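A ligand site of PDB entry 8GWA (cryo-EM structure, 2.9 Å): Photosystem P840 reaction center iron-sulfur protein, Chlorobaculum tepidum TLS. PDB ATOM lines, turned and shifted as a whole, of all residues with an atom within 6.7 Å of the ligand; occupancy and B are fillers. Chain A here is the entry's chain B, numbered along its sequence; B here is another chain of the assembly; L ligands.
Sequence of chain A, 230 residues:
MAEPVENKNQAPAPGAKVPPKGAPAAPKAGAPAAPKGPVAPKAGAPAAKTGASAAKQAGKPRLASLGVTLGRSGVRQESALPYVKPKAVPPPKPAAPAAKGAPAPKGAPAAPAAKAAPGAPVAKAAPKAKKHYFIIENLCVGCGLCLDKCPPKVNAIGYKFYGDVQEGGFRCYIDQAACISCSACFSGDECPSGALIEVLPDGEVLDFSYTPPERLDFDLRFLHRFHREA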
ATOM      1  N   PHE A 134      -8.726 -30.091  21.611  1.00  0.00           N
ATOM      2  CA  PHE A 134      -7.681 -31.062  21.292  1.00  0.00           C
ATOM      3  C   PHE A 134      -6.640 -30.544  20.294  1.00  0.00           C
ATOM      4  O   PHE A 134      -6.875 -29.558  19.585  1.00  0.00           O
ATOM      5  CB  PHE A 134      -8.296 -32.352  20.746  1.00  0.00           C
ATOM      6  CG  PHE A 134      -9.084 -33.125  21.767  1.00  0.00           C
ATOM      7  CD1 PHE A 134      -8.450 -33.954  22.666  1.00  0.00           C
ATOM      8  CD2 PHE A 134     -10.471 -33.035  21.808  1.00  0.00           C
ATOM      9  CE1 PHE A 134      -9.174 -34.671  23.601  1.00  0.00           C
ATOM     10  CE2 PHE A 134     -11.195 -33.752  22.743  1.00  0.00           C
ATOM     11  CZ  PHE A 134     -10.546 -34.564  23.643  1.00  0.00           C
ATOM     12  N   ILE A 135      -5.489 -31.194  20.254  1.00  0.00           N
ATOM     13  CA  ILE A 135      -4.490 -30.992  19.216  1.00  0.00           C
ATOM     14  C   ILE A 135      -4.004 -32.364  18.746  1.00  0.00           C
ATOM     15  O   ILE A 135      -3.591 -33.192  19.561  1.00  0.00           O
ATOM     16  CB  ILE A 135      -3.294 -30.142  19.701  1.00  0.00           C
ATOM     17  CG1 ILE A 135      -3.689 -28.676  19.801  1.00  0.00           C
ATOM     18  CG2 ILE A 135      -2.108 -30.317  18.763  1.00  0.00           C
ATOM     19  CD1 ILE A 135      -2.577 -27.790  20.308  1.00  0.00           C
ATOM     20  N   ILE A 136      -4.059 -32.582  17.439  1.00  0.00           N
ATOM     21  CA  ILE A 136      -3.551 -33.816  16.845  1.00  0.00           C
ATOM     22  C   ILE A 136      -2.027 -33.697  16.774  1.00  0.00           C
ATOM     23  O   ILE A 136      -1.511 -32.850  16.041  1.00  0.00           O
ATOM     24  CB  ILE A 136      -4.152 -34.067  15.462  1.00  0.00           C
ATOM     25  CG1 ILE A 136      -5.664 -34.178  15.535  1.00  0.00           C
ATOM     26  CG2 ILE A 136      -3.569 -35.323  14.851  1.00  0.00           C
ATOM     27  CD1 ILE A 136      -6.328 -34.221  14.171  1.00  0.00           C
ATOM     28  N   LEU A 139      -0.693 -33.766  12.682  1.00  0.00           N
ATOM     29  CA  LEU A 139      -0.586 -32.658  11.744  1.00  0.00           C
ATOM     30  C   LEU A 139       0.154 -31.473  12.324  1.00  0.00           C
ATOM     31  O   LEU A 139       0.763 -30.717  11.571  1.00  0.00           O
ATOM     32  CB  LEU A 139      -1.976 -32.200  11.286  1.00  0.00           C
ATOM     33  CG  LEU A 139      -2.642 -32.972  10.136  1.00  0.00           C
ATOM     34  CD1 LEU A 139      -1.838 -32.845   8.845  1.00  0.00           C
ATOM     35  CD2 LEU A 139      -2.891 -34.421  10.493  1.00  0.00           C
ATOM     36  N   CYS A 140       0.155 -31.321  13.648  1.00  0.00           N
ATOM     37  CA  CYS A 140       0.704 -30.140  14.279  1.00  0.00           C
ATOM     38  C   CYS A 140       2.190 -29.983  13.958  1.00  0.00           C
ATOM     39  O   CYS A 140       2.969 -30.931  14.066  1.00  0.00           O
ATOM     40  CB  CYS A 140       0.501 -30.204  15.795  1.00  0.00           C
ATOM     41  SG  CYS A 140       1.378 -28.930  16.714  1.00  0.00           S
ATOM     42  N   VAL A 141       2.566 -28.771  13.564  1.00  0.00           N
ATOM     43  CA  VAL A 141       3.952 -28.424  13.297  1.00  0.00           C
ATOM     44  C   VAL A 141       4.549 -27.603  14.428  1.00  0.00           C
ATOM     45  O   VAL A 141       5.654 -27.081  14.292  1.00  0.00           O
ATOM     46  CB  VAL A 141       4.089 -27.687  11.959  1.00  0.00           C
ATOM     47  CG1 VAL A 141       3.730 -28.618  10.809  1.00  0.00           C
ATOM     48  CG2 VAL A 141       3.211 -26.452  11.940  1.00  0.00           C
ATOM     49  N   GLY A 142       3.827 -27.468  15.538  1.00  0.00           N
ATOM     50  CA  GLY A 142       4.358 -26.812  16.712  1.00  0.00           C
ATOM     51  C   GLY A 142       4.499 -25.317  16.622  1.00  0.00           C
ATOM     52  O   GLY A 142       5.182 -24.716  17.459  1.00  0.00           O
ATOM     53  N   CYS A 143       3.870 -24.675  15.631  1.00  0.00           N
ATOM     54  CA  CYS A 143       4.032 -23.238  15.431  1.00  0.00           C
ATOM     55  C   CYS A 143       3.614 -22.446  16.668  1.00  0.00           C
ATOM     56  O   CYS A 143       4.126 -21.347  16.892  1.00  0.00           O
ATOM     57  CB  CYS A 143       3.238 -22.782  14.214  1.00  0.00           C
ATOM     58  SG  CYS A 143       1.458 -22.915  14.362  1.00  0.00           S
ATOM     59  N   GLY A 144       2.692 -22.975  17.459  1.00  0.00           N
ATOM     60  CA  GLY A 144       2.308 -22.318  18.688  1.00  0.00           C
ATOM     61  C   GLY A 144       1.334 -21.174  18.532  1.00  0.00           C
ATOM     62  O   GLY A 144       1.028 -20.510  19.529  1.00  0.00           O
ATOM     63  N   LEU A 145       0.847 -20.908  17.321  1.00  0.00           N
ATOM     64  CA  LEU A 145      -0.187 -19.894  17.150  1.00  0.00           C
ATOM     65  C   LEU A 145      -1.435 -20.237  17.953  1.00  0.00           C
ATOM     66  O   LEU A 145      -2.152 -19.334  18.409  1.00  0.00           O
ATOM     67  CB  LEU A 145      -0.538 -19.744  15.672  1.00  0.00           C
ATOM     68  CG  LEU A 145       0.635 -19.393  14.742  1.00  0.00           C
ATOM     69  CD1 LEU A 145       0.224 -19.505  13.283  1.00  0.00           C
ATOM     70  CD2 LEU A 145       1.159 -17.996  15.053  1.00  0.00           C
ATOM     71  N   CYS A 146      -1.710 -21.528  18.147  1.00  0.00           N
ATOM     72  CA  CYS A 146      -2.755 -21.937  19.072  1.00  0.00           C
ATOM     73  C   CYS A 146      -2.414 -21.536  20.502  1.00  0.00           C
ATOM     74  O   CYS A 146      -3.281 -21.074  21.247  1.00  0.00           O
ATOM     75  CB  CYS A 146      -2.977 -23.449  18.973  1.00  0.00           C
ATOM     76  SG  CYS A 146      -1.554 -24.436  19.462  1.00  0.00           S
ATOM     77  N   LEU A 147      -1.149 -21.705  20.904  1.00  0.00           N
ATOM     78  CA  LEU A 147      -0.731 -21.293  22.237  1.00  0.00           C
ATOM     79  C   LEU A 147      -0.800 -19.784  22.433  1.00  0.00           C
ATOM     80  O   LEU A 147      -1.060 -19.309  23.540  1.00  0.00           O
ATOM     81  CB  LEU A 147       0.682 -21.796  22.531  1.00  0.00           C
ATOM     82  CG  LEU A 147       1.239 -21.490  23.923  1.00  0.00           C
ATOM     83  CD1 LEU A 147       0.419 -22.145  24.998  1.00  0.00           C
ATOM     84  CD2 LEU A 147       2.676 -21.966  24.028  1.00  0.00           C
ATOM     85  N   LYS A 149      -3.071 -17.824  21.475  1.00  0.00           N
ATOM     86  CA  LYS A 149      -4.448 -17.451  21.763  1.00  0.00           C
ATOM     87  C   LYS A 149      -4.996 -18.101  23.032  1.00  0.00           C
ATOM     88  O   LYS A 149      -6.098 -17.739  23.465  1.00  0.00           O
ATOM     89  CB  LYS A 149      -5.346 -17.808  20.578  1.00  0.00           C
ATOM     90  CG  LYS A 149      -5.008 -17.036  19.313  1.00  0.00           C
ATOM     91  CD  LYS A 149      -5.952 -17.374  18.185  1.00  0.00           C
ATOM     92  CE  LYS A 149      -5.711 -18.786  17.673  1.00  0.00           C
ATOM     93  NZ  LYS A 149      -4.373 -18.922  17.025  1.00  0.00           N
ATOM     94  N   ILE A 157      -2.465 -25.286  26.530  1.00  0.00           N
ATOM     95  CA  ILE A 157      -1.587 -25.662  25.424  1.00  0.00           C
ATOM     96  C   ILE A 157      -0.142 -25.601  25.910  1.00  0.00           C
ATOM     97  O   ILE A 157       0.210 -24.742  26.733  1.00  0.00           O
ATOM     98  CB  ILE A 157      -1.816 -24.759  24.205  1.00  0.00           C
ATOM     99  CG1 ILE A 157      -3.306 -24.731  23.858  1.00  0.00           C
ATOM    100  CG2 ILE A 157      -1.004 -25.250  23.015  1.00  0.00           C
ATOM    101  CD1 ILE A 157      -3.611 -24.154  22.496  1.00  0.00           C
ATOM    102  N   TYR A 159       4.131 -27.571  25.057  1.00  0.00           N
ATOM    103  CA  TYR A 159       5.109 -28.074  24.108  1.00  0.00           C
ATOM    104  C   TYR A 159       5.706 -29.394  24.589  1.00  0.00           C
ATOM    105  O   TYR A 159       5.957 -29.574  25.790  1.00  0.00           O
ATOM    106  CB  TYR A 159       6.225 -27.053  23.885  1.00  0.00           C
ATOM    107  CG  TYR A 159       5.997 -26.113  22.723  1.00  0.00           C
ATOM    108  CD1 TYR A 159       5.474 -24.851  22.928  1.00  0.00           C
ATOM    109  CD2 TYR A 159       6.316 -26.497  21.437  1.00  0.00           C
ATOM    110  CE1 TYR A 159       5.259 -23.988  21.868  1.00  0.00           C
ATOM    111  CE2 TYR A 159       6.113 -25.638  20.370  1.00  0.00           C
ATOM    112  CZ  TYR A 159       5.591 -24.384  20.598  1.00  0.00           C
ATOM    113  OH  TYR A 159       5.385 -23.535  19.532  1.00  0.00           O
ATOM    114  N   PHE A 170       8.770 -30.483  17.934  1.00  0.00           N
ATOM    115  CA  PHE A 170       8.286 -29.540  18.925  1.00  0.00           C
ATOM    116  C   PHE A 170       6.763 -29.451  18.886  1.00  0.00           C
ATOM    117  O   PHE A 170       6.175 -28.367  18.893  1.00  0.00           O
ATOM    118  CB  PHE A 170       8.987 -28.187  18.767  1.00  0.00           C
ATOM    119  CG  PHE A 170       8.734 -27.517  17.446  1.00  0.00           C
ATOM    120  CD1 PHE A 170       9.419 -27.925  16.311  1.00  0.00           C
ATOM    121  CD2 PHE A 170       7.900 -26.415  17.358  1.00  0.00           C
ATOM    122  CE1 PHE A 170       9.215 -27.299  15.106  1.00  0.00           C
ATOM    123  CE2 PHE A 170       7.710 -25.783  16.146  1.00  0.00           C
ATOM    124  CZ  PHE A 170       8.363 -26.224  15.019  1.00  0.00           C
ATOM    125  N   ARG A 171       6.099 -30.607  18.818  1.00  0.00           N
ATOM    126  CA  ARG A 171       4.647 -30.643  18.768  1.00  0.00           C
ATOM    127  C   ARG A 171       4.024 -29.993  19.994  1.00  0.00           C
ATOM    128  O   ARG A 171       4.636 -29.891  21.068  1.00  0.00           O
ATOM    129  CB  ARG A 171       4.128 -32.075  18.644  1.00  0.00           C
ATOM    130  CG  ARG A 171       4.008 -32.578  17.222  1.00  0.00           C
ATOM    131  CD  ARG A 171       5.336 -33.083  16.722  1.00  0.00           C
ATOM    132  NE  ARG A 171       5.193 -33.922  15.543  1.00  0.00           N
ATOM    133  CZ  ARG A 171       5.098 -33.465  14.305  1.00  0.00           C
ATOM    134  NH1 ARG A 171       5.135 -32.165  14.051  1.00  0.00           N
ATOM    135  NH2 ARG A 171       4.980 -34.324  13.296  1.00  0.00           N
ATOM    136  N   CYS A 172       2.782 -29.546  19.833  1.00  0.00           N
ATOM    137  CA  CYS A 172       1.999 -28.960  20.908  1.00  0.00           C
ATOM    138  C   CYS A 172       0.888 -29.911  21.330  1.00  0.00           C
ATOM    139  O   CYS A 172       0.480 -30.798  20.591  1.00  0.00           O
ATOM    140  CB  CYS A 172       1.403 -27.615  20.475  1.00  0.00           C
ATOM    141  SG  CYS A 172       2.610 -26.283  20.276  1.00  0.00           S
ATOM    142  N   CYS A 185      -8.300 -20.811  20.557  1.00  0.00           N
ATOM    143  CA  CYS A 185      -7.300 -21.477  19.717  1.00  0.00           C
ATOM    144  C   CYS A 185      -7.884 -21.844  18.359  1.00  0.00           C
ATOM    145  O   CYS A 185      -7.197 -21.711  17.329  1.00  0.00           O
ATOM    146  CB  CYS A 185      -6.769 -22.713  20.427  1.00  0.00           C
ATOM    147  SG  CYS A 185      -8.042 -23.764  21.170  1.00  0.00           S
ATOM    148  N   GLU A 190      -6.014 -20.011  12.761  1.00  0.00           N
ATOM    149  CA  GLU A 190      -4.597 -19.903  12.482  1.00  0.00           C
ATOM    150  C   GLU A 190      -3.847 -21.228  12.396  1.00  0.00           C
ATOM    151  O   GLU A 190      -2.679 -21.218  12.010  1.00  0.00           O
ATOM    152  CB  GLU A 190      -3.899 -19.035  13.540  1.00  0.00           C
ATOM    153  CG  GLU A 190      -4.082 -17.553  13.338  1.00  0.00           C
ATOM    154  CD  GLU A 190      -3.832 -16.779  14.601  1.00  0.00           C
ATOM    155  OE1 GLU A 190      -4.782 -16.591  15.393  1.00  0.00           O
ATOM    156  OE2 GLU A 190      -2.666 -16.393  14.833  1.00  0.00           O
ATOM    157  N   CYS A 191      -4.475 -22.342  12.743  1.00  0.00           N
ATOM    158  CA  CYS A 191      -3.766 -23.614  12.656  1.00  0.00           C
ATOM    159  C   CYS A 191      -3.522 -23.931  11.189  1.00  0.00           C
ATOM    160  O   CYS A 191      -4.480 -24.165  10.440  1.00  0.00           O
ATOM    161  CB  CYS A 191      -4.566 -24.732  13.324  1.00  0.00           C
ATOM    162  SG  CYS A 191      -3.727 -26.330  13.354  1.00  0.00           S
ATOM    163  N   PRO A 192      -2.265 -23.964  10.731  1.00  0.00           N
ATOM    164  CA  PRO A 192      -2.013 -24.125   9.291  1.00  0.00           C
ATOM    165  C   PRO A 192      -2.116 -25.561   8.822  1.00  0.00           C
ATOM    166  O   PRO A 192      -2.325 -25.778   7.619  1.00  0.00           O
ATOM    167  CB  PRO A 192      -0.580 -23.613   9.134  1.00  0.00           C
ATOM    168  CG  PRO A 192       0.048 -23.951  10.451  1.00  0.00           C
ATOM    169  CD  PRO A 192      -1.022 -23.777  11.496  1.00  0.00           C
ATOM    170  N   SER A 193      -1.992 -26.530   9.717  1.00  0.00           N
ATOM    171  CA  SER A 193      -1.983 -27.934   9.359  1.00  0.00           C
ATOM    172  C   SER A 193      -3.265 -28.652   9.754  1.00  0.00           C
ATOM    173  O   SER A 193      -3.370 -29.862   9.561  1.00  0.00           O
ATOM    174  CB  SER A 193      -0.775 -28.627   9.997  1.00  0.00           C
ATOM    175  OG  SER A 193      -0.649 -28.277  11.353  1.00  0.00           O
ATOM    176  N   GLY A 194      -4.248 -27.927  10.293  1.00  0.00           N
ATOM    177  CA  GLY A 194      -5.487 -28.552  10.695  1.00  0.00           C
ATOM    178  C   GLY A 194      -5.328 -29.560  11.818  1.00  0.00           C
ATOM    179  O   GLY A 194      -5.960 -30.616  11.794  1.00  0.00           O
ATOM    180  N   ALA A 195      -4.494 -29.236  12.811  1.00  0.00           N
ATOM    181  CA  ALA A 195      -4.344 -30.102  13.969  1.00  0.00           C
ATOM    182  C   ALA A 195      -5.393 -29.818  15.032  1.00  0.00           C
ATOM    183  O   ALA A 195      -5.883 -30.743  15.691  1.00  0.00           O
ATOM    184  CB  ALA A 195      -2.947 -29.955  14.564  1.00  0.00           C
ATOM    185  N   LEU A 196      -5.748 -28.553  15.221  1.00  0.00           N
ATOM    186  CA  LEU A 196      -6.901 -28.210  16.055  1.00  0.00           C
ATOM    187  C   LEU A 196      -8.168 -28.695  15.368  1.00  0.00           C
ATOM    188  O   LEU A 196      -8.334 -28.528  14.161  1.00  0.00           O
ATOM    189  CB  LEU A 196      -6.967 -26.699  16.272  1.00  0.00           C
ATOM    190  CG  LEU A 196      -6.067 -26.144  17.369  1.00  0.00           C
ATOM    191  CD1 LEU A 196      -5.779 -24.675  17.104  1.00  0.00           C
ATOM    192  CD2 LEU A 196      -6.694 -26.334  18.733  1.00  0.00           C
ATOM    193  N   LEU B 518      -0.151 -28.125   4.914  1.00  0.00           N
ATOM    194  CA  LEU B 518      -0.139 -26.770   5.467  1.00  0.00           C
ATOM    195  C   LEU B 518      -0.913 -25.831   4.550  1.00  0.00           C
ATOM    196  O   LEU B 518      -1.153 -26.129   3.384  1.00  0.00           O
ATOM    197  CB  LEU B 518       1.292 -26.256   5.647  1.00  0.00           C
ATOM    198  CG  LEU B 518       2.203 -27.067   6.570  1.00  0.00           C
ATOM    199  CD1 LEU B 518       3.648 -26.642   6.411  1.00  0.00           C
ATOM    200  CD2 LEU B 518       1.761 -26.966   8.019  1.00  0.00           C
ATOM    201  N   LEU B 528       5.974 -20.826  10.309  1.00  0.00           N
ATOM    202  CA  LEU B 528       5.380 -21.872  11.128  1.00  0.00           C
ATOM    203  C   LEU B 528       6.398 -22.548  12.026  1.00  0.00           C
ATOM    204  O   LEU B 528       6.024 -23.372  12.868  1.00  0.00           O
ATOM    205  CB  LEU B 528       4.713 -22.940  10.253  1.00  0.00           C
ATOM    206  CG  LEU B 528       3.666 -22.453   9.265  1.00  0.00           C
ATOM    207  CD1 LEU B 528       3.018 -23.660   8.620  1.00  0.00           C
ATOM    208  CD2 LEU B 528       2.635 -21.565   9.940  1.00  0.00           C
HETATM  209 FE1  LIG L   1       0.251 -24.656  15.173  1.00  0.00          FE
HETATM  210 FE2  LIG L   1       0.089 -27.183  16.065  1.00  0.00          FE
HETATM  211 FE3  LIG L   1      -2.093 -26.020  14.895  1.00  0.00          FE
HETATM  212 FE4  LIG L   1      -1.281 -25.232  17.350  1.00  0.00          FE
HETATM  213  S1  LIG L   1      -2.057 -27.282  16.788  1.00  0.00           S
HETATM  214  S2  LIG L   1      -1.866 -23.896  15.603  1.00  0.00           S
HETATM  215  S3  LIG L   1       1.001 -25.438  17.195  1.00  0.00           S
HETATM  216  S4  LIG L   1      -0.073 -26.486  13.899  1.00  0.00           S
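OG of Ser 193 lies close to S4 of the ligand (3.2 Å).
The side-chain sulfur (SG) of Cys 146 is bound to an iron atom (FE4) of the ligand.
A sulfur (S4) of the ligand sits close to the backbone NH of Val 141.
An iron atom (FE3) of the ligand is bound by the side-chain sulfur (SG) of Cys 191 (2.3 Å).
The side-chain sulfur (SG) of Cys 143 binds an iron atom (FE1) of the ligand, 2.3 Å away.
The side-chain sulfur of Cys 172 lies close to a sulfur (S3) of the ligand.
A sulfur (S2) of the ligand sits close to the backbone NH (N) of Cys 146 (3.5 Å).
The side-chain sulfur of Cys 140 binds an iron atom (FE2) of the ligand, 2.3 Å away.
The backbone NH (N) of Gly 144 sits close to a sulfur (S3) of the ligand.
The backbone NH (N) of Cys 143 sits close to a sulfur (S3) of the ligand, at 3.4 Å.
CD1 of Ile 135 touches S1 of the ligand (3.6 Å).
Gly 142 touches the ligand.
Pro 192 touches the ligand.
Ala 195 touches the ligand (CB to S1, 3.6 Å).
Within 4 Å of the ligand: Ile 135, Cys 140, Val 141, Gly 142, Cys 143, Gly 144, Cys 146, Cys 172, Cys 191, Pro 192, Ser 193 and Ala 195.
The backbone carbonyl oxygen (O) of Ala 195 lies within hydrogen-bond range of the backbone NH (N) of Ile 136, at 3.1 Å.
The side-chain sulfur (SG) of Cys 191 lies close to the backbone NH (N) of Ala 195 (3.1 Å).
O of Cys 140 is in hydrogen-bond range of NH1 of Arg 171, 2.5 Å away.
SG of Cys 191 lies close to N of Leu 196.
SG of Cys 191 sits close to N of Gly 194.
The backbone NH of Cys 172 sits close to the side-chain sulfur of Cys 140 (3.5 Å).
OG of Ser 193 is in hydrogen-bond range of O of Leu 139, 2.8 Å away.
N of Gly 142 sits close to SG of Cys 140, 3.1 Å away.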
